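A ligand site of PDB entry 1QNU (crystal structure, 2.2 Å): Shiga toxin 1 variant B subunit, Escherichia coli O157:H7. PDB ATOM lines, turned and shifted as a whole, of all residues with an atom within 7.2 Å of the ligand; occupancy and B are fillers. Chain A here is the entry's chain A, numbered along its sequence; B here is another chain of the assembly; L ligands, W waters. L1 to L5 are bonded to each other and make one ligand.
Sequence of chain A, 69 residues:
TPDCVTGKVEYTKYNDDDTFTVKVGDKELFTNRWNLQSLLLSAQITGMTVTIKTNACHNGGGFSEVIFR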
ATOM      1  N   THR A   1       4.561 -15.182  20.745  1.00  0.00           N
ATOM      2  CA  THR A   1       5.033 -14.222  21.798  1.00  0.00           C
ATOM      3  C   THR A   1       5.615 -15.027  22.954  1.00  0.00           C
ATOM      4  O   THR A   1       4.996 -15.994  23.421  1.00  0.00           O
ATOM      5  CB  THR A   1       3.867 -13.362  22.337  1.00  0.00           C
ATOM      6  OG1 THR A   1       3.142 -12.810  21.226  1.00  0.00           O
ATOM      7  CG2 THR A   1       4.378 -12.234  23.222  1.00  0.00           C
ATOM      8  N   PRO A   2       6.806 -14.647  23.446  1.00  0.00           N
ATOM      9  CA  PRO A   2       7.427 -15.382  24.552  1.00  0.00           C
ATOM     10  C   PRO A   2       6.758 -15.178  25.918  1.00  0.00           C
ATOM     11  O   PRO A   2       6.183 -14.119  26.203  1.00  0.00           O
ATOM     12  CB  PRO A   2       8.858 -14.866  24.544  1.00  0.00           C
ATOM     13  CG  PRO A   2       8.689 -13.443  24.100  1.00  0.00           C
ATOM     14  CD  PRO A   2       7.679 -13.565  22.965  1.00  0.00           C
ATOM     15  N   THR A  19      -6.673   1.874  31.949  1.00  0.00           N
ATOM     16  CA  THR A  19      -5.910   0.666  31.653  1.00  0.00           C
ATOM     17  C   THR A  19      -5.939  -0.112  32.960  1.00  0.00           C
ATOM     18  O   THR A  19      -6.398   0.410  33.980  1.00  0.00           O
ATOM     19  CB  THR A  19      -4.428   0.932  31.207  1.00  0.00           C
ATOM     20  OG1 THR A  19      -3.734   1.653  32.229  1.00  0.00           O
ATOM     21  CG2 THR A  19      -4.397   1.693  29.894  1.00  0.00           C
ATOM     22  N   PHE A  30       0.801  -3.862  32.501  1.00  0.00           N
ATOM     23  CA  PHE A  30      -0.511  -3.291  32.265  1.00  0.00           C
ATOM     24  C   PHE A  30      -1.068  -3.728  30.908  1.00  0.00           C
ATOM     25  O   PHE A  30      -0.319  -4.121  30.025  1.00  0.00           O
ATOM     26  CB  PHE A  30      -0.460  -1.754  32.277  1.00  0.00           C
ATOM     27  CG  PHE A  30       0.030  -1.150  30.972  1.00  0.00           C
ATOM     28  CD1 PHE A  30       1.387  -0.956  30.736  1.00  0.00           C
ATOM     29  CD2 PHE A  30      -0.876  -0.768  29.977  1.00  0.00           C
ATOM     30  CE1 PHE A  30       1.837  -0.415  29.530  1.00  0.00           C
ATOM     31  CE2 PHE A  30      -0.437  -0.225  28.762  1.00  0.00           C
ATOM     32  CZ  PHE A  30       0.920  -0.044  28.544  1.00  0.00           C
ATOM     33  N   THR A  31      -2.391  -3.646  30.763  1.00  0.00           N
ATOM     34  CA  THR A  31      -3.055  -3.963  29.514  1.00  0.00           C
ATOM     35  C   THR A  31      -4.141  -2.926  29.238  1.00  0.00           C
ATOM     36  O   THR A  31      -4.792  -2.417  30.161  1.00  0.00           O
ATOM     37  CB  THR A  31      -3.690  -5.366  29.515  1.00  0.00           C
ATOM     38  OG1 THR A  31      -4.269  -5.634  28.233  1.00  0.00           O
ATOM     39  CG2 THR A  31      -4.772  -5.483  30.625  1.00  0.00           C
ATOM     40  N   ASN A  32      -4.327  -2.604  27.962  1.00  0.00           N
ATOM     41  CA  ASN A  32      -5.349  -1.644  27.554  1.00  0.00           C
ATOM     42  C   ASN A  32      -6.584  -2.349  26.999  1.00  0.00           C
ATOM     43  O   ASN A  32      -7.448  -1.697  26.436  1.00  0.00           O
ATOM     44  CB  ASN A  32      -4.799  -0.679  26.504  1.00  0.00           C
ATOM     45  CG  ASN A  32      -4.363  -1.381  25.212  1.00  0.00           C
ATOM     46  OD1 ASN A  32      -4.592  -2.580  25.015  1.00  0.00           O
ATOM     47  ND2 ASN A  32      -3.733  -0.618  24.325  1.00  0.00           N
ATOM     48  N   ARG A  33      -6.660  -3.679  27.122  1.00  0.00           N
ATOM     49  CA  ARG A  33      -7.821  -4.410  26.619  1.00  0.00           C
ATOM     50  C   ARG A  33      -8.890  -4.437  27.704  1.00  0.00           C
ATOM     51  O   ARG A  33      -8.700  -5.030  28.763  1.00  0.00           O
ATOM     52  CB  ARG A  33      -7.430  -5.845  26.202  1.00  0.00           C
ATOM     53  CG  ARG A  33      -6.257  -5.922  25.221  1.00  0.00           C
ATOM     54  CD  ARG A  33      -6.560  -5.148  23.932  1.00  0.00           C
ATOM     55  NE  ARG A  33      -5.393  -5.096  23.052  1.00  0.00           N
ATOM     56  CZ  ARG A  33      -5.073  -5.997  22.116  1.00  0.00           C
ATOM     57  NH1 ARG A  33      -5.836  -7.060  21.904  1.00  0.00           N
ATOM     58  NH2 ARG A  33      -3.980  -5.841  21.376  1.00  0.00           N
ATOM     59  N   LEU A  36     -10.177  -7.809  29.317  1.00  0.00           N
ATOM     60  CA  LEU A  36      -9.322  -8.476  30.295  1.00  0.00           C
ATOM     61  C   LEU A  36      -9.477  -8.028  31.761  1.00  0.00           C
ATOM     62  O   LEU A  36      -9.030  -8.723  32.671  1.00  0.00           O
ATOM     63  CB  LEU A  36      -7.853  -8.330  29.886  1.00  0.00           C
ATOM     64  CG  LEU A  36      -7.362  -9.267  28.778  1.00  0.00           C
ATOM     65  CD1 LEU A  36      -5.982  -8.829  28.346  1.00  0.00           C
ATOM     66  CD2 LEU A  36      -7.337 -10.721  29.296  1.00  0.00           C
ATOM     67  N   LYS A  53       2.145 -13.427  28.325  1.00  0.00           N
ATOM     68  CA  LYS A  53       3.098 -13.436  27.235  1.00  0.00           C
ATOM     69  C   LYS A  53       3.251 -12.029  26.657  1.00  0.00           C
ATOM     70  O   LYS A  53       2.261 -11.414  26.224  1.00  0.00           O
ATOM     71  CB  LYS A  53       2.617 -14.380  26.117  1.00  0.00           C
ATOM     72  CG  LYS A  53       2.499 -15.827  26.541  1.00  0.00           C
ATOM     73  CD  LYS A  53       1.722 -16.633  25.516  1.00  0.00           C
ATOM     74  CE  LYS A  53       2.620 -17.299  24.498  1.00  0.00           C
ATOM     75  NZ  LYS A  53       3.597 -18.220  25.143  1.00  0.00           N
ATOM     76  N   THR A  54       4.475 -11.511  26.639  1.00  0.00           N
ATOM     77  CA  THR A  54       4.735 -10.197  26.086  1.00  0.00           C
ATOM     78  C   THR A  54       6.228  -9.987  25.813  1.00  0.00           C
ATOM     79  O   THR A  54       7.061 -10.540  26.522  1.00  0.00           O
ATOM     80  CB  THR A  54       4.254  -9.068  27.023  1.00  0.00           C
ATOM     81  OG1 THR A  54       4.555  -7.804  26.427  1.00  0.00           O
ATOM     82  CG2 THR A  54       4.954  -9.145  28.399  1.00  0.00           C
ATOM     83  N   ASN A  55       6.550  -9.187  24.803  1.00  0.00           N
ATOM     84  CA  ASN A  55       7.933  -8.866  24.458  1.00  0.00           C
ATOM     85  C   ASN A  55       8.445  -7.730  25.355  1.00  0.00           C
ATOM     86  O   ASN A  55       9.654  -7.507  25.454  1.00  0.00           O
ATOM     87  CB  ASN A  55       8.035  -8.437  22.988  1.00  0.00           C
ATOM     88  CG  ASN A  55       8.123  -9.613  22.041  1.00  0.00           C
ATOM     89  OD1 ASN A  55       7.503  -9.612  20.975  1.00  0.00           O
ATOM     90  ND2 ASN A  55       8.894 -10.620  22.413  1.00  0.00           N
ATOM     91  N   ALA A  56       7.520  -7.022  26.000  1.00  0.00           N
ATOM     92  CA  ALA A  56       7.883  -5.932  26.895  1.00  0.00           C
ATOM     93  C   ALA A  56       7.873  -6.485  28.299  1.00  0.00           C
ATOM     94  O   ALA A  56       7.130  -6.020  29.172  1.00  0.00           O
ATOM     95  CB  ALA A  56       6.859  -4.788  26.778  1.00  0.00           C
ATOM     96  N   CYS A  57       8.710  -7.490  28.524  1.00  0.00           N
ATOM     97  CA  CYS A  57       8.773  -8.160  29.805  1.00  0.00           C
ATOM     98  C   CYS A  57       9.617  -7.442  30.848  1.00  0.00           C
ATOM     99  O   CYS A  57      10.702  -7.881  31.204  1.00  0.00           O
ATOM    100  CB  CYS A  57       9.271  -9.607  29.628  1.00  0.00           C
ATOM    101  SG  CYS A  57       9.045 -10.666  31.082  1.00  0.00           S
ATOM    102  N   HIS A  58       9.084  -6.323  31.348  1.00  0.00           N
ATOM    103  CA  HIS A  58       9.759  -5.514  32.361  1.00  0.00           C
ATOM    104  C   HIS A  58       8.658  -4.714  33.075  1.00  0.00           C
ATOM    105  O   HIS A  58       7.566  -4.553  32.536  1.00  0.00           O
ATOM    106  CB  HIS A  58      10.771  -4.565  31.695  1.00  0.00           C
ATOM    107  CG  HIS A  58      10.166  -3.704  30.617  1.00  0.00           C
ATOM    108  ND1 HIS A  58       9.428  -2.566  30.907  1.00  0.00           N
ATOM    109  CD2 HIS A  58      10.152  -3.828  29.277  1.00  0.00           C
ATOM    110  CE1 HIS A  58       8.984  -2.039  29.766  1.00  0.00           C
ATOM    111  NE2 HIS A  58       9.408  -2.788  28.769  1.00  0.00           N
ATOM    112  N   GLY A  60       6.150  -2.134  34.157  1.00  0.00           N
ATOM    113  CA  GLY A  60       5.556  -1.074  33.348  1.00  0.00           C
ATOM    114  C   GLY A  60       5.260  -1.497  31.917  1.00  0.00           C
ATOM    115  O   GLY A  60       4.591  -0.770  31.183  1.00  0.00           O
ATOM    116  N   GLY A  61       5.752  -2.666  31.498  1.00  0.00           N
ATOM    117  CA  GLY A  61       5.492  -3.131  30.135  1.00  0.00           C
ATOM    118  C   GLY A  61       4.040  -3.508  29.892  1.00  0.00           C
ATOM    119  O   GLY A  61       3.309  -3.854  30.816  1.00  0.00           O
ATOM    120  N   GLY A  62       3.593  -3.447  28.644  1.00  0.00           N
ATOM    121  CA  GLY A  62       2.212  -3.786  28.360  1.00  0.00           C
ATOM    122  C   GLY A  62       2.051  -5.198  27.828  1.00  0.00           C
ATOM    123  O   GLY A  62       3.033  -5.832  27.430  1.00  0.00           O
ATOM    124  N   PHE A  63       0.834  -5.711  27.849  1.00  0.00           N
ATOM    125  CA  PHE A  63       0.565  -7.046  27.325  1.00  0.00           C
ATOM    126  C   PHE A  63      -0.886  -7.136  26.867  1.00  0.00           C
ATOM    127  O   PHE A  63      -1.711  -6.284  27.217  1.00  0.00           O
ATOM    128  CB  PHE A  63       0.809  -8.132  28.394  1.00  0.00           C
ATOM    129  CG  PHE A  63      -0.214  -8.127  29.500  1.00  0.00           C
ATOM    130  CD1 PHE A  63      -0.107  -7.247  30.589  1.00  0.00           C
ATOM    131  CD2 PHE A  63      -1.322  -8.967  29.442  1.00  0.00           C
ATOM    132  CE1 PHE A  63      -1.079  -7.206  31.588  1.00  0.00           C
ATOM    133  CE2 PHE A  63      -2.315  -8.934  30.442  1.00  0.00           C
ATOM    134  CZ  PHE A  63      -2.183  -8.058  31.512  1.00  0.00           C
ATOM    135  N   SER A  64      -1.176  -8.166  26.093  1.00  0.00           N
ATOM    136  CA  SER A  64      -2.529  -8.439  25.647  1.00  0.00           C
ATOM    137  C   SER A  64      -2.791  -9.953  25.718  1.00  0.00           C
ATOM    138  O   SER A  64      -3.947 -10.376  25.723  1.00  0.00           O
ATOM    139  CB  SER A  64      -2.747  -7.970  24.213  1.00  0.00           C
ATOM    140  OG  SER A  64      -1.913  -8.659  23.312  1.00  0.00           O
ATOM    141  N   GLU A  65      -1.731 -10.762  25.784  1.00  0.00           N
ATOM    142  CA  GLU A  65      -1.894 -12.224  25.816  1.00  0.00           C
ATOM    143  C   GLU A  65      -1.727 -12.845  27.167  1.00  0.00           C
ATOM    144  O   GLU A  65      -0.684 -12.672  27.814  1.00  0.00           O
ATOM    145  CB  GLU A  65      -0.905 -12.885  24.849  1.00  0.00           C
ATOM    146  CG  GLU A  65      -1.099 -12.453  23.421  1.00  0.00           C
ATOM    147  CD  GLU A  65      -0.108 -13.105  22.465  1.00  0.00           C
ATOM    148  OE1 GLU A  65      -0.076 -14.354  22.401  1.00  0.00           O
ATOM    149  OE2 GLU A  65       0.623 -12.379  21.783  1.00  0.00           O
ATOM    150  N   ASP B  16      -3.931 -11.729  21.008  1.00  0.00           N
ATOM    151  CA  ASP B  16      -3.592 -10.356  20.646  1.00  0.00           C
ATOM    152  C   ASP B  16      -4.624  -9.696  19.723  1.00  0.00           C
ATOM    153  O   ASP B  16      -4.774  -8.467  19.733  1.00  0.00           O
ATOM    154  CB  ASP B  16      -2.208 -10.331  20.014  1.00  0.00           C
ATOM    155  CG  ASP B  16      -1.697  -8.911  19.773  1.00  0.00           C
ATOM    156  OD1 ASP B  16      -1.428  -8.192  20.756  1.00  0.00           O
ATOM    157  OD2 ASP B  16      -1.562  -8.537  18.596  1.00  0.00           O
ATOM    158  N   ASP B  18      -7.778 -10.110  19.999  1.00  0.00           N
ATOM    159  CA  ASP B  18      -9.021 -10.118  20.781  1.00  0.00           C
ATOM    160  C   ASP B  18      -9.912 -11.354  20.632  1.00  0.00           C
ATOM    161  O   ASP B  18     -11.074 -11.315  21.025  1.00  0.00           O
ATOM    162  CB  ASP B  18      -9.843  -8.861  20.507  1.00  0.00           C
ATOM    163  CG  ASP B  18      -9.116  -7.585  20.923  1.00  0.00           C
ATOM    164  OD1 ASP B  18      -8.739  -7.449  22.108  1.00  0.00           O
ATOM    165  OD2 ASP B  18      -8.925  -6.728  20.053  1.00  0.00           O
HETATM  166  C1  LIG L   1       9.117  -4.611  18.917  1.00  0.00           C
HETATM  167  C2  LIG L   1       8.114  -5.756  19.041  1.00  0.00           C
HETATM  168  C3  LIG L   1       6.815  -5.250  19.698  1.00  0.00           C
HETATM  169  C4  LIG L   1       7.113  -4.504  21.005  1.00  0.00           C
HETATM  170  C5  LIG L   1       8.184  -3.436  20.765  1.00  0.00           C
HETATM  171  C6  LIG L   1       8.609  -2.717  22.033  1.00  0.00           C
HETATM  172  O1  LIG L   1      10.321  -5.092  18.427  1.00  0.00           O
HETATM  173  O2  LIG L   1       7.826  -6.269  17.755  1.00  0.00           O
HETATM  174  O3  LIG L   1       5.966  -6.360  19.974  1.00  0.00           O
HETATM  175  O4  LIG L   1       5.906  -3.874  21.473  1.00  0.00           O
HETATM  176  O5  LIG L   1       9.367  -4.047  20.207  1.00  0.00           O
HETATM  177  O6  LIG L   1       8.539  -3.580  23.161  1.00  0.00           O
HETATM  178  C1  LG2 L   2       5.388  -4.323  22.684  1.00  0.00           C
HETATM  179  C2  LG2 L   2       4.481  -3.242  23.288  1.00  0.00           C
HETATM  180  C3  LG2 L   2       3.746  -3.771  24.527  1.00  0.00           C
HETATM  181  C4  LG2 L   2       3.055  -5.097  24.223  1.00  0.00           C
HETATM  182  C5  LG2 L   2       4.063  -6.078  23.615  1.00  0.00           C
HETATM  183  C6  LG2 L   2       3.468  -7.423  23.246  1.00  0.00           C
HETATM  184  O1  LG2 L   2       5.287  -2.105  23.659  1.00  0.00           O
HETATM  185  O2  LG2 L   2       2.785  -2.816  24.958  1.00  0.00           O
HETATM  186  O3  LG2 L   2       1.962  -4.875  23.308  1.00  0.00           O
HETATM  187  O4  LG2 L   2       4.624  -5.514  22.417  1.00  0.00           O
HETATM  188  O5  LG2 L   2       4.491  -8.380  22.965  1.00  0.00           O
HETATM  189  C1  LG3 L   3       0.732  -5.468  23.649  1.00  0.00           C
HETATM  190  C2  LG3 L   3      -0.224  -5.459  22.451  1.00  0.00           C
HETATM  191  C3  LG3 L   3      -0.619  -4.036  22.101  1.00  0.00           C
HETATM  192  C4  LG3 L   3      -1.263  -3.384  23.326  1.00  0.00           C
HETATM  193  C5  LG3 L   3      -0.293  -3.444  24.516  1.00  0.00           C
HETATM  194  C6  LG3 L   3      -0.888  -2.905  25.807  1.00  0.00           C
HETATM  195  O1  LG3 L   3       0.392  -6.080  21.325  1.00  0.00           O
HETATM  196  O2  LG3 L   3      -1.531  -4.034  21.016  1.00  0.00           O
HETATM  197  O3  LG3 L   3      -2.468  -4.072  23.644  1.00  0.00           O
HETATM  198  O4  LG3 L   3       0.122  -4.812  24.767  1.00  0.00           O
HETATM  199  O5  LG3 L   3      -1.934  -3.739  26.286  1.00  0.00           O
HETATM  200  C1  LG4 L   4       5.608  -1.010  22.767  1.00  0.00           C
HETATM  201  C2  LG4 L   4       4.648   0.117  23.132  1.00  0.00           C
HETATM  202  O1  LG4 L   4       3.270  -0.192  22.683  1.00  0.00           O
HETATM  203  C3  LG4 L   4       2.333   0.315  23.488  1.00  0.00           C
HETATM  204  O2  LG4 L   4       2.460   1.187  24.348  1.00  0.00           O
HETATM  205  N1  LG4 L   4       1.141  -0.049  23.002  1.00  0.00           N
HETATM  206  C4  LG4 L   4      -0.135   0.423  23.519  1.00  0.00           C
HETATM  207  C1  LG5 L   5      -0.644   0.993  22.197  1.00  0.00           C
HETATM  208  O1  LG5 L   5      -1.237  -0.266  21.691  1.00  0.00           O
HETATM  209  C2  LG5 L   5      -2.181  -0.075  20.755  1.00  0.00           C
HETATM  210  O2  LG5 L   5      -2.826   0.938  20.525  1.00  0.00           O
HETATM  211  N1  LG5 L   5      -2.492  -1.260  20.233  1.00  0.00           N
HETATM  212  C3  LG5 L   5      -3.593  -1.482  19.303  1.00  0.00           C
HETATM  213  C4  LG5 L   5      -4.683  -2.368  19.901  1.00  0.00           C
HETATM  214  O   HOH W   1       2.802  -5.076  20.064  1.00  0.00           O
HETATM  215  O   HOH W   2       1.132  -9.419  24.893  1.00  0.00           O
HETATM  216  O   HOH W   3       4.985  -1.341  26.806  1.00  0.00           O
HETATM  217  O   HOH W   4       3.589  -9.247  20.664  1.00  0.00           O
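O of Phe 63 sits at hydrogen-bond distance from OG1 of Thr 31.
The guanidinium group (NE) of Arg 33 is in hydrogen-bond range of the side-chain amide oxygen (OD1) of Asn 32, 3.3 Å away.
The side-chain hydroxyl of Thr 31 sits at hydrogen-bond distance from the backbone NH of Arg 33, 3.3 Å away.
The backbone carbonyl oxygen (O) of Gly 62 sits at hydrogen-bond distance from the side-chain hydroxyl (OG1) of Thr 54 (2.7 Å).
N of Ala 56 lies within hydrogen-bond range of OG1 of Thr 54 (3.1 Å).
The backbone carbonyl oxygen (O) of Pro 2 lies within hydrogen-bond range of the backbone NH (N) of Thr 54 (3.1 Å).
The backbone carbonyl oxygen (O) of Thr 1 lies close to the side-chain amino group (NZ) of Lys 53, at 3.1 Å.
The side-chain carboxylate (OE2) of Glu 65 is in hydrogen-bond range of the side-chain hydroxyl (OG1) of Thr 1.
O4 of LG3 L3 lies within hydrogen-bond range of N of Phe 63, at 3.3 Å.
An oxygen (O5) of LG3 L3 sits at hydrogen-bond distance from the backbone carbonyl oxygen (O) of Phe 63, 2.7 Å away.
An oxygen (O1) of LG3 L3 is in hydrogen-bond range of the side-chain carboxylate (OD1) of Asp 16 of chain B, 2.8 Å away.
The backbone NH (N) of Asn 55 sits at hydrogen-bond distance from an oxygen (O5) of LG2 L2 (2.9 Å).
The backbone NH (N) of Asn 32 lies within hydrogen-bond range of an oxygen (O5) of LG3 L3 (3.1 Å).
An oxygen (O3) of LG3 L3 is in hydrogen-bond range of the side-chain amide oxygen of Asn 32, 2.9 Å away.
The guanidinium group (NH2) of Arg 33 is in hydrogen-bond range of an oxygen (O2) of LG3 L3, at 3.1 Å.
CG2 of Thr 1 touches O5 of LG2 L2, at 3.9 Å.
CA of Thr 31 touches O5 of LG3 L3 (3.4 Å).
OG1 of Thr 54 touches C5 of LG2 L2, 3.3 Å away.
CB of Ala 56 touches C3 of LG2 L2 (3.97 Å).
Gly 62 touches the ligand.
OG of Ser 64 touches C2 of LG3 L3 (3.7 Å).
Within 4 Å of the ligand: Thr 1, Thr 31, Asn 32, Arg 33, Thr 54, Asn 55, Ala 56, Gly 62, Phe 63, Ser 64 and Asp 16 of chain B.
Along chain A the residues within 4 Å of the ligand span positions 1 to 64.
Water W3 lies within hydrogen-bond range of N of Gly 62 and O2 of LG2 L2.
Water W2 lies within hydrogen-bond range of the backbone carbonyl oxygen (O) of Lys 53 (2.7 Å), the backbone NH (N) of Ser 64 (2.9 Å) and the backbone NH (N) of Glu 65 (3.3 Å).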
